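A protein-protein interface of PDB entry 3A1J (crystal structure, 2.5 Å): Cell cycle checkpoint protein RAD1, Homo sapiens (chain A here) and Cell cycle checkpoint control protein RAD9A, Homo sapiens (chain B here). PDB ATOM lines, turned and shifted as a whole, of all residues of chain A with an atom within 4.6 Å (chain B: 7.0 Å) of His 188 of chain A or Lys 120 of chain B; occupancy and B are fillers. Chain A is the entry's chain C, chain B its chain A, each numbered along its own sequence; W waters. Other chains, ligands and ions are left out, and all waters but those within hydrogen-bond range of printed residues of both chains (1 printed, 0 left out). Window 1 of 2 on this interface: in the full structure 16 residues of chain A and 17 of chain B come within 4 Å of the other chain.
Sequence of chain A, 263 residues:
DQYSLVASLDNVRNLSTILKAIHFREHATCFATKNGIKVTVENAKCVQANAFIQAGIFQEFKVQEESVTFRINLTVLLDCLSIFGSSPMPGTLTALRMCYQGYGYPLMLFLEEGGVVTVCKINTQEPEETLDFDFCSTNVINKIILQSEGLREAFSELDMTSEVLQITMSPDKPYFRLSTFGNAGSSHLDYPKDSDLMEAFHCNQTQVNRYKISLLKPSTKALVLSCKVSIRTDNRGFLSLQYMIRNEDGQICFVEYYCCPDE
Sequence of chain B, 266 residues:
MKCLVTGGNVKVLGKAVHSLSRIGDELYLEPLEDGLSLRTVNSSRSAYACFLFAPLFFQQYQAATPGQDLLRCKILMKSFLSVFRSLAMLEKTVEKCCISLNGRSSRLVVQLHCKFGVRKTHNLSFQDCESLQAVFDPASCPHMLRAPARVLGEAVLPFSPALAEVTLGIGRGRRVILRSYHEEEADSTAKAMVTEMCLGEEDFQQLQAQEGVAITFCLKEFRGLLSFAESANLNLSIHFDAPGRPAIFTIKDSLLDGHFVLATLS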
ATOM      1  N   GLU A 157      13.801  18.969 -21.106  1.00  0.00           N
ATOM      2  CA  GLU A 157      13.610  17.759 -21.901  1.00  0.00           C
ATOM      3  C   GLU A 157      12.175  17.572 -22.389  1.00  0.00           C
ATOM      4  O   GLU A 157      11.755  16.458 -22.714  1.00  0.00           O
ATOM      5  CB  GLU A 157      14.072  16.522 -21.120  1.00  0.00           C
ATOM      6  CG  GLU A 157      15.587  16.343 -21.131  1.00  0.00           C
ATOM      7  CD  GLU A 157      16.164  16.402 -22.543  1.00  0.00           C
ATOM      8  OE1 GLU A 157      15.750  15.578 -23.389  1.00  0.00           O
ATOM      9  OE2 GLU A 157      17.024  17.273 -22.811  1.00  0.00           O
ATOM     10  N   ARG A 177       0.561  17.332 -13.837  1.00  0.00           N
ATOM     11  CA  ARG A 177       1.089  16.663 -15.025  1.00  0.00           C
ATOM     12  C   ARG A 177       1.299  17.520 -16.273  1.00  0.00           C
ATOM     13  O   ARG A 177       0.396  18.218 -16.725  1.00  0.00           O
ATOM     14  CB  ARG A 177       0.188  15.489 -15.404  1.00  0.00           C
ATOM     15  CG  ARG A 177       0.334  15.065 -16.867  1.00  0.00           C
ATOM     16  CD  ARG A 177      -0.476  13.825 -17.198  1.00  0.00           C
ATOM     17  NE  ARG A 177      -0.088  12.708 -16.344  1.00  0.00           N
ATOM     18  CZ  ARG A 177      -0.621  11.492 -16.412  1.00  0.00           C
ATOM     19  NH1 ARG A 177      -1.568  11.227 -17.300  1.00  0.00           N
ATOM     20  NH2 ARG A 177      -0.205  10.547 -15.583  1.00  0.00           N
ATOM     21  N   LEU A 178       2.500  17.440 -16.834  1.00  0.00           N
ATOM     22  CA  LEU A 178       2.827  18.166 -18.054  1.00  0.00           C
ATOM     23  C   LEU A 178       2.886  17.100 -19.136  1.00  0.00           C
ATOM     24  O   LEU A 178       3.590  16.099 -18.999  1.00  0.00           O
ATOM     25  CB  LEU A 178       4.190  18.856 -17.951  1.00  0.00           C
ATOM     26  CG  LEU A 178       4.470  19.880 -16.849  1.00  0.00           C
ATOM     27  CD1 LEU A 178       3.322  20.868 -16.759  1.00  0.00           C
ATOM     28  CD2 LEU A 178       4.678  19.167 -15.535  1.00  0.00           C
ATOM     29  N   SER A 179       2.143  17.301 -20.212  1.00  0.00           N
ATOM     30  CA  SER A 179       2.132  16.313 -21.273  1.00  0.00           C
ATOM     31  C   SER A 179       2.362  16.928 -22.641  1.00  0.00           C
ATOM     32  O   SER A 179       1.918  18.049 -22.922  1.00  0.00           O
ATOM     33  CB  SER A 179       0.796  15.572 -21.268  1.00  0.00           C
ATOM     34  OG  SER A 179       0.460  15.134 -19.964  1.00  0.00           O
ATOM     35  N   SER A 186       3.632  10.153 -27.195  1.00  0.00           N
ATOM     36  CA  SER A 186       2.822  10.747 -26.141  1.00  0.00           C
ATOM     37  C   SER A 186       3.701  10.648 -24.903  1.00  0.00           C
ATOM     38  O   SER A 186       4.215   9.580 -24.589  1.00  0.00           O
ATOM     39  CB  SER A 186       1.539   9.943 -25.934  1.00  0.00           C
ATOM     40  OG  SER A 186       0.771  10.465 -24.870  1.00  0.00           O
ATOM     41  N   SER A 187       3.885  11.755 -24.198  1.00  0.00           N
ATOM     42  CA  SER A 187       4.737  11.742 -23.021  1.00  0.00           C
ATOM     43  C   SER A 187       4.122  12.496 -21.842  1.00  0.00           C
ATOM     44  O   SER A 187       3.368  13.451 -22.039  1.00  0.00           O
ATOM     45  CB  SER A 187       6.088  12.339 -23.393  1.00  0.00           C
ATOM     46  OG  SER A 187       6.943  12.384 -22.276  1.00  0.00           O
ATOM     47  N   HIS A 188       4.435  12.063 -20.620  1.00  0.00           N
ATOM     48  CA  HIS A 188       3.899  12.706 -19.419  1.00  0.00           C
ATOM     49  C   HIS A 188       4.943  12.909 -18.338  1.00  0.00           C
ATOM     50  O   HIS A 188       5.822  12.070 -18.145  1.00  0.00           O
ATOM     51  CB  HIS A 188       2.757  11.885 -18.822  1.00  0.00           C
ATOM     52  CG  HIS A 188       1.695  11.518 -19.809  1.00  0.00           C
ATOM     53  ND1 HIS A 188       1.538  10.236 -20.289  1.00  0.00           N
ATOM     54  CD2 HIS A 188       0.775  12.277 -20.451  1.00  0.00           C
ATOM     55  CE1 HIS A 188       0.570  10.222 -21.189  1.00  0.00           C
ATOM     56  NE2 HIS A 188       0.091  11.448 -21.307  1.00  0.00           N
ATOM     57  N   LEU A 189       4.837  14.029 -17.632  1.00  0.00           N
ATOM     58  CA  LEU A 189       5.751  14.350 -16.536  1.00  0.00           C
ATOM     59  C   LEU A 189       4.866  14.519 -15.306  1.00  0.00           C
ATOM     60  O   LEU A 189       4.025  15.416 -15.254  1.00  0.00           O
ATOM     61  CB  LEU A 189       6.521  15.637 -16.846  1.00  0.00           C
ATOM     62  CG  LEU A 189       7.652  16.096 -15.920  1.00  0.00           C
ATOM     63  CD1 LEU A 189       8.585  14.939 -15.570  1.00  0.00           C
ATOM     64  CD2 LEU A 189       8.429  17.204 -16.621  1.00  0.00           C
ATOM     65  N   ASP A 190       5.049  13.644 -14.326  1.00  0.00           N
ATOM     66  CA  ASP A 190       4.236  13.666 -13.114  1.00  0.00           C
ATOM     67  C   ASP A 190       4.943  14.052 -11.827  1.00  0.00           C
ATOM     68  O   ASP A 190       6.008  13.524 -11.508  1.00  0.00           O
ATOM     69  CB  ASP A 190       3.594  12.294 -12.897  1.00  0.00           C
ATOM     70  CG  ASP A 190       2.601  11.932 -13.979  1.00  0.00           C
ATOM     71  OD1 ASP A 190       2.188  10.755 -14.010  1.00  0.00           O
ATOM     72  OD2 ASP A 190       2.228  12.810 -14.787  1.00  0.00           O
ATOM     73  N   SER B  82      15.390  10.334 -27.734  1.00  0.00           N
ATOM     74  CA  SER B  82      14.905  11.448 -26.918  1.00  0.00           C
ATOM     75  C   SER B  82      14.743  11.010 -25.464  1.00  0.00           C
ATOM     76  O   SER B  82      15.001  11.787 -24.546  1.00  0.00           O
ATOM     77  CB  SER B  82      13.566  11.978 -27.439  1.00  0.00           C
ATOM     78  OG  SER B  82      12.514  11.059 -27.201  1.00  0.00           O
ATOM     79  N   VAL B  83      14.323   9.762 -25.252  1.00  0.00           N
ATOM     80  CA  VAL B  83      14.141   9.248 -23.896  1.00  0.00           C
ATOM     81  C   VAL B  83      15.434   9.333 -23.100  1.00  0.00           C
ATOM     82  O   VAL B  83      15.413   9.701 -21.925  1.00  0.00           O
ATOM     83  CB  VAL B  83      13.671   7.771 -23.891  1.00  0.00           C
ATOM     84  CG1 VAL B  83      13.633   7.245 -22.467  1.00  0.00           C
ATOM     85  CG2 VAL B  83      12.294   7.659 -24.516  1.00  0.00           C
ATOM     86  N   MET B  89      20.943  14.338 -17.198  1.00  0.00           N
ATOM     87  CA  MET B  89      19.678  14.183 -16.492  1.00  0.00           C
ATOM     88  C   MET B  89      19.481  12.735 -16.058  1.00  0.00           C
ATOM     89  O   MET B  89      18.767  12.458 -15.096  1.00  0.00           O
ATOM     90  CB  MET B  89      18.531  14.651 -17.398  1.00  0.00           C
ATOM     91  CG  MET B  89      17.137  14.561 -16.795  1.00  0.00           C
ATOM     92  SD  MET B  89      16.172  12.992 -17.410  1.00  0.00           S
ATOM     93  CE  MET B  89      15.297  13.759 -18.962  1.00  0.00           C
ATOM     94  N   ARG B 107       1.321   1.133 -28.049  1.00  0.00           N
ATOM     95  CA  ARG B 107       2.519   1.906 -27.781  1.00  0.00           C
ATOM     96  C   ARG B 107       3.499   1.130 -26.913  1.00  0.00           C
ATOM     97  O   ARG B 107       3.105   0.241 -26.162  1.00  0.00           O
ATOM     98  CB  ARG B 107       2.135   3.195 -27.059  1.00  0.00           C
ATOM     99  CG  ARG B 107       1.117   4.054 -27.788  1.00  0.00           C
ATOM    100  CD  ARG B 107       0.630   5.170 -26.869  1.00  0.00           C
ATOM    101  NE  ARG B 107      -0.123   6.209 -27.569  1.00  0.00           N
ATOM    102  CZ  ARG B 107      -0.581   7.317 -26.989  1.00  0.00           C
ATOM    103  NH1 ARG B 107      -0.365   7.532 -25.698  1.00  0.00           N
ATOM    104  NH2 ARG B 107      -1.250   8.214 -27.700  1.00  0.00           N
ATOM    105  N   VAL B 110       8.090   3.442 -21.943  1.00  0.00           N
ATOM    106  CA  VAL B 110       9.354   3.640 -21.256  1.00  0.00           C
ATOM    107  C   VAL B 110       9.035   4.619 -20.138  1.00  0.00           C
ATOM    108  O   VAL B 110       8.612   5.748 -20.380  1.00  0.00           O
ATOM    109  CB  VAL B 110      10.429   4.245 -22.161  1.00  0.00           C
ATOM    110  CG1 VAL B 110      11.683   4.502 -21.349  1.00  0.00           C
ATOM    111  CG2 VAL B 110      10.733   3.304 -23.307  1.00  0.00           C
ATOM    112  N   GLN B 111       9.242   4.174 -18.911  1.00  0.00           N
ATOM    113  CA  GLN B 111       8.936   4.987 -17.757  1.00  0.00           C
ATOM    114  C   GLN B 111      10.148   5.192 -16.859  1.00  0.00           C
ATOM    115  O   GLN B 111      10.669   4.237 -16.288  1.00  0.00           O
ATOM    116  CB  GLN B 111       7.805   4.302 -17.001  1.00  0.00           C
ATOM    117  CG  GLN B 111       7.328   4.981 -15.746  1.00  0.00           C
ATOM    118  CD  GLN B 111       6.038   4.357 -15.256  1.00  0.00           C
ATOM    119  OE1 GLN B 111       5.886   3.136 -15.279  1.00  0.00           O
ATOM    120  NE2 GLN B 111       5.102   5.190 -14.807  1.00  0.00           N
ATOM    121  N   LEU B 112      10.610   6.435 -16.752  1.00  0.00           N
ATOM    122  CA  LEU B 112      11.753   6.727 -15.892  1.00  0.00           C
ATOM    123  C   LEU B 112      11.256   7.096 -14.503  1.00  0.00           C
ATOM    124  O   LEU B 112      10.434   8.002 -14.351  1.00  0.00           O
ATOM    125  CB  LEU B 112      12.596   7.888 -16.434  1.00  0.00           C
ATOM    126  CG  LEU B 112      13.326   7.824 -17.784  1.00  0.00           C
ATOM    127  CD1 LEU B 112      13.901   6.435 -18.029  1.00  0.00           C
ATOM    128  CD2 LEU B 112      12.364   8.200 -18.888  1.00  0.00           C
ATOM    129  N   HIS B 113      11.730   6.376 -13.495  1.00  0.00           N
ATOM    130  CA  HIS B 113      11.350   6.660 -12.119  1.00  0.00           C
ATOM    131  C   HIS B 113      12.453   7.552 -11.572  1.00  0.00           C
ATOM    132  O   HIS B 113      13.573   7.095 -11.332  1.00  0.00           O
ATOM    133  CB  HIS B 113      11.240   5.365 -11.316  1.00  0.00           C
ATOM    134  CG  HIS B 113      10.100   4.495 -11.744  1.00  0.00           C
ATOM    135  ND1 HIS B 113       8.781   4.846 -11.545  1.00  0.00           N
ATOM    136  CD2 HIS B 113      10.078   3.311 -12.402  1.00  0.00           C
ATOM    137  CE1 HIS B 113       7.997   3.918 -12.066  1.00  0.00           C
ATOM    138  NE2 HIS B 113       8.759   2.976 -12.593  1.00  0.00           N
ATOM    139  N   CYS B 114      12.126   8.829 -11.386  1.00  0.00           N
ATOM    140  CA  CYS B 114      13.091   9.823 -10.914  1.00  0.00           C
ATOM    141  C   CYS B 114      13.046  10.166  -9.430  1.00  0.00           C
ATOM    142  O   CYS B 114      12.120   9.793  -8.718  1.00  0.00           O
ATOM    143  CB  CYS B 114      12.919  11.104 -11.726  1.00  0.00           C
ATOM    144  SG  CYS B 114      12.903  10.810 -13.491  1.00  0.00           S
ATOM    145  N   GLY B 117      10.125  11.199  -6.159  1.00  0.00           N
ATOM    146  CA  GLY B 117       8.858  10.691  -6.650  1.00  0.00           C
ATOM    147  C   GLY B 117       8.432  11.168  -8.024  1.00  0.00           C
ATOM    148  O   GLY B 117       7.320  10.873  -8.470  1.00  0.00           O
ATOM    149  N   VAL B 118       9.296  11.906  -8.710  1.00  0.00           N
ATOM    150  CA  VAL B 118       8.946  12.385 -10.040  1.00  0.00           C
ATOM    151  C   VAL B 118       8.953  11.200 -10.995  1.00  0.00           C
ATOM    152  O   VAL B 118       9.793  10.298 -10.884  1.00  0.00           O
ATOM    153  CB  VAL B 118       9.937  13.459 -10.537  1.00  0.00           C
ATOM    154  CG1 VAL B 118       9.534  13.933 -11.925  1.00  0.00           C
ATOM    155  CG2 VAL B 118       9.956  14.627  -9.564  1.00  0.00           C
ATOM    156  N   ARG B 119       8.018  11.203 -11.939  1.00  0.00           N
ATOM    157  CA  ARG B 119       7.922  10.110 -12.888  1.00  0.00           C
ATOM    158  C   ARG B 119       7.707  10.634 -14.298  1.00  0.00           C
ATOM    159  O   ARG B 119       6.917  11.554 -14.516  1.00  0.00           O
ATOM    160  CB  ARG B 119       6.762   9.200 -12.484  1.00  0.00           C
ATOM    161  CG  ARG B 119       6.962   7.741 -12.816  1.00  0.00           C
ATOM    162  CD  ARG B 119       5.826   6.910 -12.247  1.00  0.00           C
ATOM    163  NE  ARG B 119       4.559   7.190 -12.919  1.00  0.00           N
ATOM    164  CZ  ARG B 119       3.377   6.744 -12.504  1.00  0.00           C
ATOM    165  NH1 ARG B 119       3.295   5.995 -11.411  1.00  0.00           N
ATOM    166  NH2 ARG B 119       2.280   7.040 -13.188  1.00  0.00           N
ATOM    167  N   LYS B 120       8.420  10.066 -15.260  1.00  0.00           N
ATOM    168  CA  LYS B 120       8.250  10.498 -16.638  1.00  0.00           C
ATOM    169  C   LYS B 120       7.910   9.293 -17.484  1.00  0.00           C
ATOM    170  O   LYS B 120       8.676   8.336 -17.534  1.00  0.00           O
ATOM    171  CB  LYS B 120       9.520  11.151 -17.188  1.00  0.00           C
ATOM    172  CG  LYS B 120       9.282  11.858 -18.520  1.00  0.00           C
ATOM    173  CD  LYS B 120      10.568  12.344 -19.172  1.00  0.00           C
ATOM    174  CE  LYS B 120      10.268  13.147 -20.445  1.00  0.00           C
ATOM    175  NZ  LYS B 120      11.500  13.385 -21.279  1.00  0.00           N
ATOM    176  N   THR B 121       6.762   9.345 -18.149  1.00  0.00           N
ATOM    177  CA  THR B 121       6.321   8.248 -19.001  1.00  0.00           C
ATOM    178  C   THR B 121       6.332   8.625 -20.477  1.00  0.00           C
ATOM    179  O   THR B 121       5.778   9.653 -20.887  1.00  0.00           O
ATOM    180  CB  THR B 121       4.901   7.772 -18.622  1.00  0.00           C
ATOM    181  OG1 THR B 121       4.913   7.258 -17.283  1.00  0.00           O
ATOM    182  CG2 THR B 121       4.441   6.674 -19.561  1.00  0.00           C
ATOM    183  N   HIS B 122       6.977   7.772 -21.264  1.00  0.00           N
ATOM    184  CA  HIS B 122       7.098   7.944 -22.701  1.00  0.00           C
ATOM    185  C   HIS B 122       6.361   6.809 -23.379  1.00  0.00           C
ATOM    186  O   HIS B 122       6.666   5.640 -23.139  1.00  0.00           O
ATOM    187  CB  HIS B 122       8.559   7.883 -23.108  1.00  0.00           C
ATOM    188  CG  HIS B 122       9.349   9.084 -22.706  1.00  0.00           C
ATOM    189  ND1 HIS B 122       9.354  10.249 -23.442  1.00  0.00           N
ATOM    190  CD2 HIS B 122      10.169   9.299 -21.651  1.00  0.00           C
ATOM    191  CE1 HIS B 122      10.145  11.130 -22.860  1.00  0.00           C
ATOM    192  NE2 HIS B 122      10.653  10.579 -21.771  1.00  0.00           N
ATOM    193  N   ASN B 123       5.390   7.159 -24.220  1.00  0.00           N
ATOM    194  CA  ASN B 123       4.602   6.173 -24.956  1.00  0.00           C
ATOM    195  C   ASN B 123       5.057   6.192 -26.403  1.00  0.00           C
ATOM    196  O   ASN B 123       4.597   7.015 -27.190  1.00  0.00           O
ATOM    197  CB  ASN B 123       3.108   6.512 -24.892  1.00  0.00           C
ATOM    198  CG  ASN B 123       2.550   6.445 -23.482  1.00  0.00           C
ATOM    199  OD1 ASN B 123       2.640   5.412 -22.810  1.00  0.00           O
ATOM    200  ND2 ASN B 123       1.965   7.548 -23.028  1.00  0.00           N
HETATM  201  O   HOH W   1       4.363   9.716 -15.991  1.00  0.00           O
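The guanidinium group (NH1) of Arg 107 of chain B sits close to the side-chain hydroxyl (OG) of Ser 186 of chain A, 3.3 Å away. NH2 of Arg 119 of chain B is in salt-bridge range of OD1 of Asp 190 of chain A. The side-chain amino group (NZ) of Lys 120 of chain B sits at hydrogen-bond distance from the backbone carbonyl oxygen (O) of Glu 157 of chain A (3.4 Å). The backbone carbonyl oxygen of Thr 121 of chain B lies close to the side-chain hydroxyl of Ser 187 of chain A. The backbone carbonyl oxygen (O) of Thr 121 of chain B is in hydrogen-bond range of the backbone NH (N) of His 188 of chain A (2.8 Å). OG of Ser 187 of chain A lies within hydrogen-bond range of ND1 of His 122 of chain B (3.4 Å). The backbone NH (N) of Asn 123 of chain B lies within hydrogen-bond range of the backbone carbonyl oxygen (O) of Ser 186 of chain A (2.7 Å).
The backbone NH (N) of His 122 of chain B sits at hydrogen-bond distance from the backbone carbonyl oxygen (O) of Val 110 of chain B (2.7 Å). NE of Arg 119 of chain B lies close to NE2 of Gln 111 of chain B (2.8 Å). NE2 of Gln 111 of chain B sits at hydrogen-bond distance from OG1 of Thr 121 of chain B, 3.2 Å away. N of Leu 112 of chain B sits at hydrogen-bond distance from O of Lys 120 of chain B (2.8 Å). The side-chain amino group of Lys 120 of chain B sits close to a ring nitrogen (NE2) of His 122 of chain B, 3.0 Å away. O of Leu 178 of chain A sits at hydrogen-bond distance from N of Leu 189 of chain A (2.8 Å).
Met 89 of chain B touches Glu 157 of chain A. His 122 of chain B touches Ser 186 of chain A. Ser 187 of chain A touches Lys 120 of chain B (OG to CE, 3.9 Å). O of His 188 of chain A touches O of Arg 119 of chain B, at 3.8 Å. Lys 120 of chain B touches His 188 of chain A. His 188 of chain A touches Asn 123 of chain B. Val 118 of chain B touches Leu 189 of chain A. Leu 189 of chain A touches Arg 119 of chain B (CA to O, 3.6 Å). Asp 190 of chain A touches Val 118 of chain B (O to CA, 3.5 Å).
Arg 177 of chain A touches none of the printed residues of chain B. Of chain B, only Arg 119 (3.8 Å), Lys 120 (3.3 Å), Thr 121 (2.8 Å) and Asn 123 (3.5 Å) come within 4 Å of His 188 of chain A. Of the printed residues of chain A, Met 89 of chain B touches Glu 157 (3.4 Å). Of the printed residues of chain A, Arg 107 of chain B touches Ser 186. His 113 of chain B touches none of the printed residues of chain A. Of the printed residues of chain A, Thr 121 of chain B touches Ser 187 (3.2 Å) and His 188 (2.8 Å).
Of the 9 printed residues of chain A, 6 touch a printed residue of chain B. Hydrophobic or aromatic side chains of chain A that line the printed part of chain B: His 188 and Leu 189. Hydrophobic or aromatic side chains of chain B that line the printed part of chain A: Met 89, Val 118 and His 122. Along chain B the printed residues that touch a printed residue of chain A span positions 89 to 123.
Water W1 lies within hydrogen-bond range of the side-chain hydroxyl (OG1) of Thr 121 of chain B (2.8 Å), the side-chain carboxylate (OD1) of Asp 190 of chain A (3.1 Å) and the backbone carbonyl oxygen (O) of Arg 119 of chain B (3.5 Å).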
